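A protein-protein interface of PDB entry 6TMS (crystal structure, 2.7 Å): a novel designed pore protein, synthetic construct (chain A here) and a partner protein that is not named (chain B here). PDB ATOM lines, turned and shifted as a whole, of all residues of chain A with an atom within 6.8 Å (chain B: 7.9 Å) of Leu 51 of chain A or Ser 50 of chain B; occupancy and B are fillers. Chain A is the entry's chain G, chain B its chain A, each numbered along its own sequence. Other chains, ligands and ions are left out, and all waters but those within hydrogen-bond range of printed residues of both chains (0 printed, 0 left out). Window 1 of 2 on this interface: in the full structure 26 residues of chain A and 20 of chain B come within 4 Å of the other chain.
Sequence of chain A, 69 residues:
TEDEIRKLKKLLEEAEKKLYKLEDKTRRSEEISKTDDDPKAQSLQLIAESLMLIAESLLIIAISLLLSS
The backbone carbonyl oxygen of Leu 51 of chain A sits at hydrogen-bond distance from the side-chain hydroxyl of Ser 50 of chain B (3.1 Å).
The side-chain hydroxyl (OG) of Ser 50 of chain B lies within hydrogen-bond range of the backbone NH (N) of Met 52 of chain A.
Leu 46 of chain B touches Leu 22 of chain A (O to CD2, 3.9 Å).
CB of Glu 49 of chain B touches CD2 of Leu 22 of chain A, 3.3 Å away.
Leu 22 of chain A touches Ser 50 of chain B (CD2 to N, 3.9 Å).
Ile 47 of chain B touches Ile 47 of chain A (CG1 to CG2, 3.8 Å).
Ile 47 of chain B touches Ala 48 of chain A (CG1 to CB, 3.96 Å).
Leu 51 of chain A touches Ile 47 of chain B.
Leu 51 of chain A touches two residues of chain B.
Ser 50 of chain B touches just these residues of chain A: Leu 22 (3.9 Å), Leu 51 (3.1 Å) and Met 52 (3.3 Å).
Of the printed residues of chain B, Leu 22 of chain A touches Leu 46 (3.9 Å), Glu 49 (3.3 Å) and Ser 50 (3.9 Å).
Of the printed residues of chain B, Met 52 of chain A touches Ser 50.
Printed residues of chain B within 4 Å of Ala 48 of chain A: Ile 47 (3.96 Å).
Ile 54 of chain A touches none of the printed residues of chain B.
The nearest residue of chain B that does not touch Leu 51 of chain A is Leu 51 of chain B (4.6 Å).
The nearest residue of chain A that does not touch Ser 50 of chain B is Ala 55 of chain A (4.2 Å).
The nearest printed residue of chain B that does not touch Leu 22 of chain A is Leu 53 of chain B (4.5 Å).
Along chain A the printed residues that touch a printed residue of chain B span positions 22 to 52.
Printed residues of chain B that touch a printed residue of chain A: Leu 46, Ile 47, Glu 49 and Ser 50.
Hydrophobic or aromatic side chains of chain B within 4 Å of the printed part of chain A: Ile 47.
Among the printed residues, 8 pairs touch across the chains.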
ATOM      1  N   LEU A  19     -21.023   3.000   4.608  1.00  0.00           N
ATOM      2  CA  LEU A  19     -19.932   2.169   4.085  1.00  0.00           C
ATOM      3  C   LEU A  19     -20.080   2.041   2.592  1.00  0.00           C
ATOM      4  O   LEU A  19     -19.106   2.048   1.828  1.00  0.00           O
ATOM      5  CB  LEU A  19     -19.959   0.762   4.690  1.00  0.00           C
ATOM      6  CG  LEU A  19     -18.863  -0.202   4.197  1.00  0.00           C
ATOM      7  CD1 LEU A  19     -17.500   0.275   4.682  1.00  0.00           C
ATOM      8  CD2 LEU A  19     -19.100  -1.635   4.616  1.00  0.00           C
ATOM      9  N   LEU A  22     -19.131   5.177   0.769  1.00  0.00           N
ATOM     10  CA  LEU A  22     -17.720   5.365   0.552  1.00  0.00           C
ATOM     11  C   LEU A  22     -17.146   4.288  -0.340  1.00  0.00           C
ATOM     12  O   LEU A  22     -16.063   4.457  -0.888  1.00  0.00           O
ATOM     13  CB  LEU A  22     -17.018   5.455   1.890  1.00  0.00           C
ATOM     14  CG  LEU A  22     -15.934   6.519   1.730  1.00  0.00           C
ATOM     15  CD1 LEU A  22     -16.588   7.912   1.585  1.00  0.00           C
ATOM     16  CD2 LEU A  22     -14.893   6.488   2.835  1.00  0.00           C
ATOM     17  N   GLU A  23     -17.796   3.151  -0.429  1.00  0.00           N
ATOM     18  CA  GLU A  23     -17.315   2.163  -1.357  1.00  0.00           C
ATOM     19  C   GLU A  23     -17.540   2.641  -2.778  1.00  0.00           C
ATOM     20  O   GLU A  23     -16.625   2.566  -3.596  1.00  0.00           O
ATOM     21  CB  GLU A  23     -17.947   0.832  -0.983  1.00  0.00           C
ATOM     22  CG  GLU A  23     -16.937   0.202  -0.054  1.00  0.00           C
ATOM     23  CD  GLU A  23     -17.370  -0.949   0.766  1.00  0.00           C
ATOM     24  OE1 GLU A  23     -18.518  -1.402   0.707  1.00  0.00           O
ATOM     25  OE2 GLU A  23     -16.519  -1.356   1.566  1.00  0.00           O
ATOM     26  N   LEU A  46      -4.172   1.892  -2.100  1.00  0.00           N
ATOM     27  CA  LEU A  46      -4.118   0.563  -1.530  1.00  0.00           C
ATOM     28  C   LEU A  46      -4.525   0.510  -0.060  1.00  0.00           C
ATOM     29  O   LEU A  46      -5.236  -0.405   0.382  1.00  0.00           O
ATOM     30  CB  LEU A  46      -2.665   0.199  -1.659  1.00  0.00           C
ATOM     31  CG  LEU A  46      -1.978  -0.955  -2.315  1.00  0.00           C
ATOM     32  CD1 LEU A  46      -1.078  -0.439  -3.459  1.00  0.00           C
ATOM     33  CD2 LEU A  46      -1.174  -1.592  -1.198  1.00  0.00           C
ATOM     34  N   ILE A  47      -4.020   1.457   0.721  1.00  0.00           N
ATOM     35  CA  ILE A  47      -4.294   1.500   2.149  1.00  0.00           C
ATOM     36  C   ILE A  47      -5.763   1.740   2.378  1.00  0.00           C
ATOM     37  O   ILE A  47      -6.372   1.213   3.312  1.00  0.00           O
ATOM     38  CB  ILE A  47      -3.477   2.650   2.768  1.00  0.00           C
ATOM     39  CG1 ILE A  47      -2.061   2.236   3.134  1.00  0.00           C
ATOM     40  CG2 ILE A  47      -4.183   3.283   3.987  1.00  0.00           C
ATOM     41  CD1 ILE A  47      -1.031   3.338   2.891  1.00  0.00           C
ATOM     42  N   ALA A  48      -6.316   2.617   1.549  1.00  0.00           N
ATOM     43  CA  ALA A  48      -7.696   3.060   1.627  1.00  0.00           C
ATOM     44  C   ALA A  48      -8.671   1.947   1.313  1.00  0.00           C
ATOM     45  O   ALA A  48      -9.789   1.909   1.847  1.00  0.00           O
ATOM     46  CB  ALA A  48      -7.845   4.177   0.618  1.00  0.00           C
ATOM     47  N   GLU A  49      -8.313   1.158   0.308  1.00  0.00           N
ATOM     48  CA  GLU A  49      -9.040  -0.048  -0.039  1.00  0.00           C
ATOM     49  C   GLU A  49      -8.950  -1.065   1.087  1.00  0.00           C
ATOM     50  O   GLU A  49      -9.897  -1.819   1.359  1.00  0.00           O
ATOM     51  CB  GLU A  49      -8.456  -0.566  -1.350  1.00  0.00           C
ATOM     52  CG  GLU A  49      -9.420  -0.363  -2.519  1.00  0.00           C
ATOM     53  CD  GLU A  49      -8.825  -0.460  -3.923  1.00  0.00           C
ATOM     54  OE1 GLU A  49      -9.393  -1.214  -4.748  1.00  0.00           O
ATOM     55  OE2 GLU A  49      -7.851   0.257  -4.223  1.00  0.00           O
ATOM     56  N   SER A  50      -7.790  -1.130   1.719  1.00  0.00           N
ATOM     57  CA  SER A  50      -7.628  -2.058   2.818  1.00  0.00           C
ATOM     58  C   SER A  50      -8.503  -1.620   3.988  1.00  0.00           C
ATOM     59  O   SER A  50      -9.197  -2.432   4.617  1.00  0.00           O
ATOM     60  CB  SER A  50      -6.142  -2.104   3.169  1.00  0.00           C
ATOM     61  OG  SER A  50      -5.846  -3.116   4.108  1.00  0.00           O
ATOM     62  N   LEU A  51      -8.583  -0.309   4.181  1.00  0.00           N
ATOM     63  CA  LEU A  51      -9.367   0.282   5.251  1.00  0.00           C
ATOM     64  C   LEU A  51     -10.843   0.139   4.972  1.00  0.00           C
ATOM     65  O   LEU A  51     -11.659  -0.059   5.877  1.00  0.00           O
ATOM     66  CB  LEU A  51      -9.038   1.765   5.352  1.00  0.00           C
ATOM     67  CG  LEU A  51      -7.913   2.213   6.271  1.00  0.00           C
ATOM     68  CD1 LEU A  51      -7.776   3.707   6.233  1.00  0.00           C
ATOM     69  CD2 LEU A  51      -8.200   1.776   7.669  1.00  0.00           C
ATOM     70  N   MET A  52     -11.196   0.237   3.715  1.00  0.00           N
ATOM     71  CA  MET A  52     -12.563   0.028   3.314  1.00  0.00           C
ATOM     72  C   MET A  52     -12.970  -1.403   3.606  1.00  0.00           C
ATOM     73  O   MET A  52     -14.099  -1.682   4.033  1.00  0.00           O
ATOM     74  CB  MET A  52     -12.616   0.337   1.828  1.00  0.00           C
ATOM     75  CG  MET A  52     -13.631   1.341   1.335  1.00  0.00           C
ATOM     76  SD  MET A  52     -13.497   3.046   1.848  1.00  0.00           S
ATOM     77  CE  MET A  52     -15.044   3.006   2.744  1.00  0.00           C
ATOM     78  N   LEU A  53     -12.030  -2.322   3.438  1.00  0.00           N
ATOM     79  CA  LEU A  53     -12.345  -3.714   3.703  1.00  0.00           C
ATOM     80  C   LEU A  53     -12.500  -3.971   5.199  1.00  0.00           C
ATOM     81  O   LEU A  53     -13.419  -4.687   5.623  1.00  0.00           O
ATOM     82  CB  LEU A  53     -11.252  -4.582   3.083  1.00  0.00           C
ATOM     83  CG  LEU A  53     -11.602  -5.913   2.393  1.00  0.00           C
ATOM     84  CD1 LEU A  53     -11.649  -7.012   3.421  1.00  0.00           C
ATOM     85  CD2 LEU A  53     -12.906  -5.882   1.618  1.00  0.00           C
ATOM     86  N   ILE A  54     -11.646  -3.369   6.026  1.00  0.00           N
ATOM     87  CA  ILE A  54     -11.855  -3.603   7.445  1.00  0.00           C
ATOM     88  C   ILE A  54     -13.133  -2.916   7.887  1.00  0.00           C
ATOM     89  O   ILE A  54     -13.810  -3.398   8.791  1.00  0.00           O
ATOM     90  CB  ILE A  54     -10.620  -3.238   8.316  1.00  0.00           C
ATOM     91  CG1 ILE A  54     -11.013  -2.858   9.749  1.00  0.00           C
ATOM     92  CG2 ILE A  54      -9.711  -2.131   7.737  1.00  0.00           C
ATOM     93  CD1 ILE A  54     -10.689  -3.895  10.783  1.00  0.00           C
ATOM     94  N   ALA A  55     -13.495  -1.783   7.313  1.00  0.00           N
ATOM     95  CA  ALA A  55     -14.753  -1.219   7.767  1.00  0.00           C
ATOM     96  C   ALA A  55     -15.893  -2.161   7.419  1.00  0.00           C
ATOM     97  O   ALA A  55     -16.767  -2.428   8.247  1.00  0.00           O
ATOM     98  CB  ALA A  55     -14.959   0.167   7.178  1.00  0.00           C
ATOM     99  N   GLU A  56     -15.851  -2.752   6.233  1.00  0.00           N
ATOM    100  CA  GLU A  56     -16.861  -3.745   5.898  1.00  0.00           C
ATOM    101  C   GLU A  56     -16.911  -4.858   6.940  1.00  0.00           C
ATOM    102  O   GLU A  56     -17.967  -5.172   7.501  1.00  0.00           O
ATOM    103  CB  GLU A  56     -16.530  -4.284   4.511  1.00  0.00           C
ATOM    104  CG  GLU A  56     -17.598  -5.120   3.841  1.00  0.00           C
ATOM    105  CD  GLU A  56     -17.467  -5.088   2.331  1.00  0.00           C
ATOM    106  OE1 GLU A  56     -16.581  -4.357   1.851  1.00  0.00           O
ATOM    107  OE2 GLU A  56     -18.331  -5.652   1.625  1.00  0.00           O
ATOM    108  N   SER B  43      -6.936  10.612  -1.719  1.00  0.00           N
ATOM    109  CA  SER B  43      -6.927   9.298  -1.106  1.00  0.00           C
ATOM    110  C   SER B  43      -6.910   9.407   0.405  1.00  0.00           C
ATOM    111  O   SER B  43      -7.557   8.621   1.093  1.00  0.00           O
ATOM    112  CB  SER B  43      -5.736   8.503  -1.616  1.00  0.00           C
ATOM    113  OG  SER B  43      -5.794   7.166  -1.160  1.00  0.00           O
ATOM    114  N   LEU B  44      -6.212  10.401   0.937  1.00  0.00           N
ATOM    115  CA  LEU B  44      -6.167  10.604   2.381  1.00  0.00           C
ATOM    116  C   LEU B  44      -7.529  10.983   2.906  1.00  0.00           C
ATOM    117  O   LEU B  44      -7.881  10.683   4.050  1.00  0.00           O
ATOM    118  CB  LEU B  44      -5.173  11.711   2.721  1.00  0.00           C
ATOM    119  CG  LEU B  44      -3.677  11.435   2.966  1.00  0.00           C
ATOM    120  CD1 LEU B  44      -2.871  12.723   2.944  1.00  0.00           C
ATOM    121  CD2 LEU B  44      -3.439  10.746   4.323  1.00  0.00           C
ATOM    122  N   GLN B  45      -8.257  11.748   2.126  1.00  0.00           N
ATOM    123  CA  GLN B  45      -9.587  12.090   2.551  1.00  0.00           C
ATOM    124  C   GLN B  45     -10.408  10.817   2.651  1.00  0.00           C
ATOM    125  O   GLN B  45     -11.117  10.597   3.640  1.00  0.00           O
ATOM    126  CB  GLN B  45     -10.159  13.100   1.562  1.00  0.00           C
ATOM    127  CG  GLN B  45     -11.668  13.248   1.591  1.00  0.00           C
ATOM    128  CD  GLN B  45     -12.347  13.307   0.214  1.00  0.00           C
ATOM    129  OE1 GLN B  45     -12.761  12.277  -0.306  1.00  0.00           O
ATOM    130  NE2 GLN B  45     -12.514  14.509  -0.343  1.00  0.00           N
ATOM    131  N   LEU B  46     -10.229   9.906   1.706  1.00  0.00           N
ATOM    132  CA  LEU B  46     -10.933   8.636   1.834  1.00  0.00           C
ATOM    133  C   LEU B  46     -10.424   7.842   3.028  1.00  0.00           C
ATOM    134  O   LEU B  46     -11.169   7.067   3.634  1.00  0.00           O
ATOM    135  CB  LEU B  46     -10.770   7.859   0.549  1.00  0.00           C
ATOM    136  CG  LEU B  46     -11.488   8.526  -0.627  1.00  0.00           C
ATOM    137  CD1 LEU B  46     -10.683   8.324  -1.907  1.00  0.00           C
ATOM    138  CD2 LEU B  46     -12.901   7.956  -0.807  1.00  0.00           C
ATOM    139  N   ILE B  47      -9.139   7.955   3.331  1.00  0.00           N
ATOM    140  CA  ILE B  47      -8.578   7.209   4.443  1.00  0.00           C
ATOM    141  C   ILE B  47      -9.187   7.677   5.756  1.00  0.00           C
ATOM    142  O   ILE B  47      -9.591   6.873   6.610  1.00  0.00           O
ATOM    143  CB  ILE B  47      -7.049   7.402   4.426  1.00  0.00           C
ATOM    144  CG1 ILE B  47      -6.350   6.331   3.590  1.00  0.00           C
ATOM    145  CG2 ILE B  47      -6.459   7.456   5.838  1.00  0.00           C
ATOM    146  CD1 ILE B  47      -5.180   6.879   2.787  1.00  0.00           C
ATOM    147  N   ALA B  48      -9.309   8.985   5.921  1.00  0.00           N
ATOM    148  CA  ALA B  48      -9.873   9.489   7.155  1.00  0.00           C
ATOM    149  C   ALA B  48     -11.325   9.079   7.248  1.00  0.00           C
ATOM    150  O   ALA B  48     -11.801   8.630   8.302  1.00  0.00           O
ATOM    151  CB  ALA B  48      -9.712  11.005   7.207  1.00  0.00           C
ATOM    152  N   GLU B  49     -12.013   9.132   6.113  1.00  0.00           N
ATOM    153  CA  GLU B  49     -13.416   8.765   6.094  1.00  0.00           C
ATOM    154  C   GLU B  49     -13.604   7.301   6.518  1.00  0.00           C
ATOM    155  O   GLU B  49     -14.457   6.982   7.366  1.00  0.00           O
ATOM    156  CB  GLU B  49     -13.957   9.090   4.684  1.00  0.00           C
ATOM    157  CG  GLU B  49     -15.321   9.863   4.656  1.00  0.00           C
ATOM    158  CD  GLU B  49     -15.514  10.986   3.573  1.00  0.00           C
ATOM    159  OE1 GLU B  49     -16.658  11.103   3.044  1.00  0.00           O
ATOM    160  OE2 GLU B  49     -14.578  11.779   3.301  1.00  0.00           O
ATOM    161  N   SER B  50     -12.743   6.413   6.033  1.00  0.00           N
ATOM    162  CA  SER B  50     -12.878   4.997   6.357  1.00  0.00           C
ATOM    163  C   SER B  50     -12.583   4.751   7.827  1.00  0.00           C
ATOM    164  O   SER B  50     -13.232   3.942   8.510  1.00  0.00           O
ATOM    165  CB  SER B  50     -11.922   4.226   5.458  1.00  0.00           C
ATOM    166  OG  SER B  50     -12.333   2.893   5.291  1.00  0.00           O
ATOM    167  N   LEU B  51     -11.659   5.532   8.333  1.00  0.00           N
ATOM    168  CA  LEU B  51     -11.189   5.399   9.692  1.00  0.00           C
ATOM    169  C   LEU B  51     -12.273   5.712  10.682  1.00  0.00           C
ATOM    170  O   LEU B  51     -12.477   5.028  11.691  1.00  0.00           O
ATOM    171  CB  LEU B  51     -10.136   6.471   9.837  1.00  0.00           C
ATOM    172  CG  LEU B  51      -9.165   6.391  10.968  1.00  0.00           C
ATOM    173  CD1 LEU B  51      -8.276   5.170  10.700  1.00  0.00           C
ATOM    174  CD2 LEU B  51      -8.401   7.730  11.105  1.00  0.00           C
ATOM    175  N   MET B  52     -12.962   6.765  10.369  1.00  0.00           N
ATOM    176  CA  MET B  52     -14.055   7.271  11.136  1.00  0.00           C
ATOM    177  C   MET B  52     -15.188   6.285  11.152  1.00  0.00           C
ATOM    178  O   MET B  52     -15.981   6.225  12.094  1.00  0.00           O
ATOM    179  CB  MET B  52     -14.349   8.558  10.426  1.00  0.00           C
ATOM    180  CG  MET B  52     -15.496   9.251  10.762  1.00  0.00           C
ATOM    181  SD  MET B  52     -16.414   9.499   9.241  1.00  0.00           S
ATOM    182  CE  MET B  52     -15.285  10.502   8.339  1.00  0.00           C
ATOM    183  N   LEU B  53     -15.311   5.559  10.074  1.00  0.00           N
ATOM    184  CA  LEU B  53     -16.303   4.516  10.027  1.00  0.00           C
ATOM    185  C   LEU B  53     -15.959   3.330  10.889  1.00  0.00           C
ATOM    186  O   LEU B  53     -16.866   2.642  11.362  1.00  0.00           O
ATOM    187  CB  LEU B  53     -16.395   4.073   8.614  1.00  0.00           C
ATOM    188  CG  LEU B  53     -17.126   5.096   7.816  1.00  0.00           C
ATOM    189  CD1 LEU B  53     -16.965   4.738   6.370  1.00  0.00           C
ATOM    190  CD2 LEU B  53     -18.558   4.898   8.269  1.00  0.00           C
ATOM    191  N   ILE B  54     -14.688   2.933  10.939  1.00  0.00           N
ATOM    192  CA  ILE B  54     -14.438   1.833  11.859  1.00  0.00           C
ATOM    193  C   ILE B  54     -14.490   2.390  13.261  1.00  0.00           C
ATOM    194  O   ILE B  54     -14.729   1.651  14.209  1.00  0.00           O
ATOM    195  CB  ILE B  54     -13.189   0.943  11.576  1.00  0.00           C
ATOM    196  CG1 ILE B  54     -12.546   0.386  12.877  1.00  0.00           C
ATOM    197  CG2 ILE B  54     -12.206   1.455  10.469  1.00  0.00           C
ATOM    198  CD1 ILE B  54     -11.451   1.160  13.564  1.00  0.00           C
ATOM    199  N   ALA B  55     -14.249   3.673  13.431  1.00  0.00           N
ATOM    200  CA  ALA B  55     -14.509   4.252  14.731  1.00  0.00           C
ATOM    201  C   ALA B  55     -15.980   4.091  15.048  1.00  0.00           C
ATOM    202  O   ALA B  55     -16.365   3.692  16.156  1.00  0.00           O
ATOM    203  CB  ALA B  55     -14.111   5.721  14.704  1.00  0.00           C
ATOM    204  N   GLU B  56     -16.806   4.322  14.037  1.00  0.00           N
ATOM    205  CA  GLU B  56     -18.236   4.121  14.141  1.00  0.00           C
ATOM    206  C   GLU B  56     -18.575   2.688  14.532  1.00  0.00           C
ATOM    207  O   GLU B  56     -19.346   2.451  15.470  1.00  0.00           O
ATOM    208  CB  GLU B  56     -18.868   4.483  12.797  1.00  0.00           C
ATOM    209  CG  GLU B  56     -20.384   4.584  12.857  1.00  0.00           C
ATOM    210  CD  GLU B  56     -21.038   5.004  11.550  1.00  0.00           C
ATOM    211  OE1 GLU B  56     -20.296   5.402  10.636  1.00  0.00           O
ATOM    212  OE2 GLU B  56     -22.296   5.028  11.475  1.00  0.00           O
ATOM    213  N   SER B  57     -18.028   1.714  13.832  1.00  0.00           N
ATOM    214  CA  SER B  57     -18.451   0.374  14.178  1.00  0.00           C
ATOM    215  C   SER B  57     -17.817  -0.111  15.460  1.00  0.00           C
ATOM    216  O   SER B  57     -18.415  -0.927  16.153  1.00  0.00           O
ATOM    217  CB  SER B  57     -18.218  -0.602  13.055  1.00  0.00           C
ATOM    218  OG  SER B  57     -19.305  -1.512  13.117  1.00  0.00           O
